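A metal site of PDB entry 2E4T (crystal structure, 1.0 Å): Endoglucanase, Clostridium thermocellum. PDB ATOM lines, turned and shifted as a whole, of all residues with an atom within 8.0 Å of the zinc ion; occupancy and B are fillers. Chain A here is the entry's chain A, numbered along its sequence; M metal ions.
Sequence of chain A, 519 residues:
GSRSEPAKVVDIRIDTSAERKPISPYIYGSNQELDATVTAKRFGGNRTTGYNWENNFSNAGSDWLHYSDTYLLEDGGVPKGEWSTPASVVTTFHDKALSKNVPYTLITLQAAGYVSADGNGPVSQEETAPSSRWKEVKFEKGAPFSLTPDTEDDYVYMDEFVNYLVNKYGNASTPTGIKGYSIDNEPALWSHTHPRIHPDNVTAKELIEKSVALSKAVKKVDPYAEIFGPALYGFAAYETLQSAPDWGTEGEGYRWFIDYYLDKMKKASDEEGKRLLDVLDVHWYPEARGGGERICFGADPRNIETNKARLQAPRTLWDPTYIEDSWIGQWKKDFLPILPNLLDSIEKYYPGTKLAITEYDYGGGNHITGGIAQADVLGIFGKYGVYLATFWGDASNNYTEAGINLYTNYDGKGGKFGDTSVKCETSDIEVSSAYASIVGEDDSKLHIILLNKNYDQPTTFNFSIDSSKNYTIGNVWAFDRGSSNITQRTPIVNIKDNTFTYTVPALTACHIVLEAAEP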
ATOM      1  N   GLU A  33     -10.735  17.815  21.982  1.00  0.00           N
ATOM      2  CA  GLU A  33     -10.654  19.255  21.766  1.00  0.00           C
ATOM      3  C   GLU A  33      -9.236  19.568  21.276  1.00  0.00           C
ATOM      4  O   GLU A  33      -8.267  19.526  22.047  1.00  0.00           O
ATOM      5  CB  GLU A  33     -10.968  20.006  23.070  1.00  0.00           C
ATOM      6  CG  GLU A  33     -12.430  19.789  23.475  1.00  0.00           C
ATOM      7  CD  GLU A  33     -12.845  20.422  24.794  1.00  0.00           C
ATOM      8  OE1 GLU A  33     -12.004  20.647  25.688  1.00  0.00           O
ATOM      9  OE2 GLU A  33     -14.077  20.705  24.940  1.00  0.00           O
ATOM     10  N   LEU A  34      -9.122  19.858  19.979  1.00  0.00           N
ATOM     11  CA  LEU A  34      -7.837  20.073  19.322  1.00  0.00           C
ATOM     12  C   LEU A  34      -7.553  21.550  19.071  1.00  0.00           C
ATOM     13  O   LEU A  34      -8.457  22.370  18.907  1.00  0.00           O
ATOM     14  CB  LEU A  34      -7.776  19.368  17.975  1.00  0.00           C
ATOM     15  CG  LEU A  34      -7.867  17.840  18.013  1.00  0.00           C
ATOM     16  CD1 LEU A  34      -7.679  17.287  16.576  1.00  0.00           C
ATOM     17  CD2 LEU A  34      -6.857  17.232  18.954  1.00  0.00           C
ATOM     18  N   ASP A  35      -6.245  21.819  18.912  1.00  0.00           N
ATOM     19  CA  ASP A  35      -5.753  23.084  18.387  1.00  0.00           C
ATOM     20  C   ASP A  35      -5.758  23.022  16.855  1.00  0.00           C
ATOM     21  O   ASP A  35      -4.721  23.031  16.177  1.00  0.00           O
ATOM     22  CB  ASP A  35      -4.329  23.314  18.856  1.00  0.00           C
ATOM     23  CG  ASP A  35      -4.179  23.131  20.348  1.00  0.00           C
ATOM     24  OD1 ASP A  35      -4.980  23.743  21.109  1.00  0.00           O
ATOM     25  OD2 ASP A  35      -3.223  22.427  20.816  1.00  0.00           O
ATOM     26  N   ALA A  36      -6.961  22.880  16.306  1.00  0.00           N
ATOM     27  CA  ALA A  36      -7.132  22.790  14.852  1.00  0.00           C
ATOM     28  C   ALA A  36      -8.558  23.202  14.573  1.00  0.00           C
ATOM     29  O   ALA A  36      -9.468  23.046  15.419  1.00  0.00           O
ATOM     30  CB  ALA A  36      -6.924  21.369  14.344  1.00  0.00           C
ATOM     31  N   GLY A 365       2.460  12.067  16.467  1.00  0.00           N
ATOM     32  CA  GLY A 365       1.631  13.281  16.287  1.00  0.00           C
ATOM     33  C   GLY A 365       2.372  14.561  16.592  1.00  0.00           C
ATOM     34  O   GLY A 365       1.933  15.642  16.176  1.00  0.00           O
ATOM     35  N   ASP A 394      -5.077  13.760  21.542  1.00  0.00           N
ATOM     36  CA  ASP A 394      -5.204  15.050  22.216  1.00  0.00           C
ATOM     37  C   ASP A 394      -4.425  16.187  21.538  1.00  0.00           C
ATOM     38  O   ASP A 394      -3.782  16.014  20.480  1.00  0.00           O
ATOM     39  CB  ASP A 394      -4.898  14.908  23.711  1.00  0.00           C
ATOM     40  CG  ASP A 394      -3.458  14.710  24.007  1.00  0.00           C
ATOM     41  OD1 ASP A 394      -2.588  15.054  23.154  1.00  0.00           O
ATOM     42  OD2 ASP A 394      -3.168  14.224  25.144  1.00  0.00           O
ATOM     43  N   ALA A 395      -4.500  17.360  22.166  1.00  0.00           N
ATOM     44  CA  ALA A 395      -3.971  18.587  21.600  1.00  0.00           C
ATOM     45  C   ALA A 395      -2.454  18.651  21.609  1.00  0.00           C
ATOM     46  O   ALA A 395      -1.860  19.603  21.076  1.00  0.00           O
ATOM     47  CB  ALA A 395      -4.570  19.782  22.348  1.00  0.00           C
ATOM     48  N   SER A 396      -1.787  17.635  22.196  1.00  0.00           N
ATOM     49  CA  SER A 396      -0.329  17.579  22.132  1.00  0.00           C
ATOM     50  C   SER A 396       0.187  17.098  20.771  1.00  0.00           C
ATOM     51  O   SER A 396       1.392  17.128  20.507  1.00  0.00           O
ATOM     52  CB  SER A 396       0.256  16.707  23.237  1.00  0.00           C
ATOM     53  OG  SER A 396       0.023  15.338  22.997  1.00  0.00           O
ATOM     54  N   ASN A 397      -0.721  16.617  19.913  1.00  0.00           N
ATOM     55  CA  ASN A 397      -0.355  16.138  18.573  1.00  0.00           C
ATOM     56  C   ASN A 397      -0.271  17.316  17.604  1.00  0.00           C
ATOM     57  O   ASN A 397      -1.136  17.494  16.709  1.00  0.00           O
ATOM     58  CB  ASN A 397      -1.369  15.094  18.108  1.00  0.00           C
ATOM     59  CG  ASN A 397      -1.326  13.849  18.949  1.00  0.00           C
ATOM     60  OD1 ASN A 397      -0.439  13.042  18.782  1.00  0.00           O
ATOM     61  ND2 ASN A 397      -2.347  13.645  19.805  1.00  0.00           N
ATOM     62  N   ASN A 398       0.739  18.151  17.811  1.00  0.00           N
ATOM     63  CA  ASN A 398       0.818  19.441  17.081  1.00  0.00           C
ATOM     64  C   ASN A 398       0.980  19.252  15.569  1.00  0.00           C
ATOM     65  O   ASN A 398       0.471  20.056  14.796  1.00  0.00           O
ATOM     66  CB  ASN A 398       1.936  20.334  17.642  1.00  0.00           C
ATOM     67  CG  ASN A 398       3.281  19.655  17.674  1.00  0.00           C
ATOM     68  OD1 ASN A 398       3.448  18.580  18.285  1.00  0.00           O
ATOM     69  ND2 ASN A 398       4.309  20.289  17.073  1.00  0.00           N
ATOM     70  N   TYR A 399       1.781  18.252  15.151  1.00  0.00           N
ATOM     71  CA  TYR A 399       1.908  17.985  13.721  1.00  0.00           C
ATOM     72  C   TYR A 399       0.636  17.379  13.143  1.00  0.00           C
ATOM     73  O   TYR A 399       0.256  17.719  12.010  1.00  0.00           O
ATOM     74  CB  TYR A 399       3.163  17.191  13.397  1.00  0.00           C
ATOM     75  CG  TYR A 399       4.391  18.053  13.289  1.00  0.00           C
ATOM     76  CD1 TYR A 399       4.612  18.791  12.133  1.00  0.00           C
ATOM     77  CD2 TYR A 399       5.323  18.152  14.329  1.00  0.00           C
ATOM     78  CE1 TYR A 399       5.763  19.607  12.007  1.00  0.00           C
ATOM     79  CE2 TYR A 399       6.466  18.955  14.211  1.00  0.00           C
ATOM     80  CZ  TYR A 399       6.688  19.662  13.044  1.00  0.00           C
ATOM     81  OH  TYR A 399       7.829  20.431  12.953  1.00  0.00           O
ATOM     82  N   THR A 400      -0.071  16.495  13.885  1.00  0.00           N
ATOM     83  CA  THR A 400      -1.353  16.030  13.377  1.00  0.00           C
ATOM     84  C   THR A 400      -2.279  17.225  13.160  1.00  0.00           C
ATOM     85  O   THR A 400      -3.020  17.312  12.156  1.00  0.00           O
ATOM     86  CB  THR A 400      -1.993  15.057  14.398  1.00  0.00           C
ATOM     87  OG1 THR A 400      -1.040  14.111  14.827  1.00  0.00           O
ATOM     88  CG2 THR A 400      -3.235  14.418  13.839  1.00  0.00           C
ATOM     89  N   GLU A 401      -2.282  18.149  14.125  1.00  0.00           N
ATOM     90  CA  GLU A 401      -3.129  19.331  14.032  1.00  0.00           C
ATOM     91  C   GLU A 401      -2.784  20.186  12.833  1.00  0.00           C
ATOM     92  O   GLU A 401      -3.664  20.717  12.136  1.00  0.00           O
ATOM     93  CB  GLU A 401      -3.018  20.137  15.337  1.00  0.00           C
ATOM     94  CG  GLU A 401      -3.685  19.411  16.486  1.00  0.00           C
ATOM     95  CD  GLU A 401      -3.364  20.040  17.851  1.00  0.00           C
ATOM     96  OE1 GLU A 401      -2.221  20.593  18.045  1.00  0.00           O
ATOM     97  OE2 GLU A 401      -4.218  19.951  18.775  1.00  0.00           O
ATOM     98  N   ALA A 402      -1.465  20.360  12.547  1.00  0.00           N
ATOM     99  CA  ALA A 402      -1.036  21.084  11.354  1.00  0.00           C
ATOM    100  C   ALA A 402      -1.580  20.366  10.099  1.00  0.00           C
ATOM    101  O   ALA A 402      -1.970  21.020   9.130  1.00  0.00           O
ATOM    102  CB  ALA A 402       0.457  21.176  11.303  1.00  0.00           C
ATOM    103  N   SER A 484       5.649  23.189  13.229  1.00  0.00           N
ATOM    104  CA  SER A 484       4.302  22.789  12.873  1.00  0.00           C
ATOM    105  C   SER A 484       3.386  23.970  12.595  1.00  0.00           C
ATOM    106  O   SER A 484       2.268  23.747  12.106  1.00  0.00           O
ATOM    107  CB  SER A 484       3.735  21.868  13.953  1.00  0.00           C
ATOM    108  OG  SER A 484       3.779  22.464  15.237  1.00  0.00           O
HETATM  109 ZN    ZN M   1      -2.043  21.180  19.880  1.00  0.00          ZN
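Three residues have an atom within 4 Å of the zinc ion: Asp 35, Ala 395 and Glu 401.
The nearest printed residue that does not touch the zinc ion is Ser 396 (4.2 Å).
The zinc ion is bound by the side-chain carboxylate (OE1) of Glu 401, the side-chain carboxylate (OD2) of Asp 35 and the backbone carbonyl oxygen (O) of Ala 395.
The zinc ion has three donor atoms within binding distance.
Slightly farther from the zinc ion lies the side-chain carboxylate (OE2) of Glu 401 (2.7 Å).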
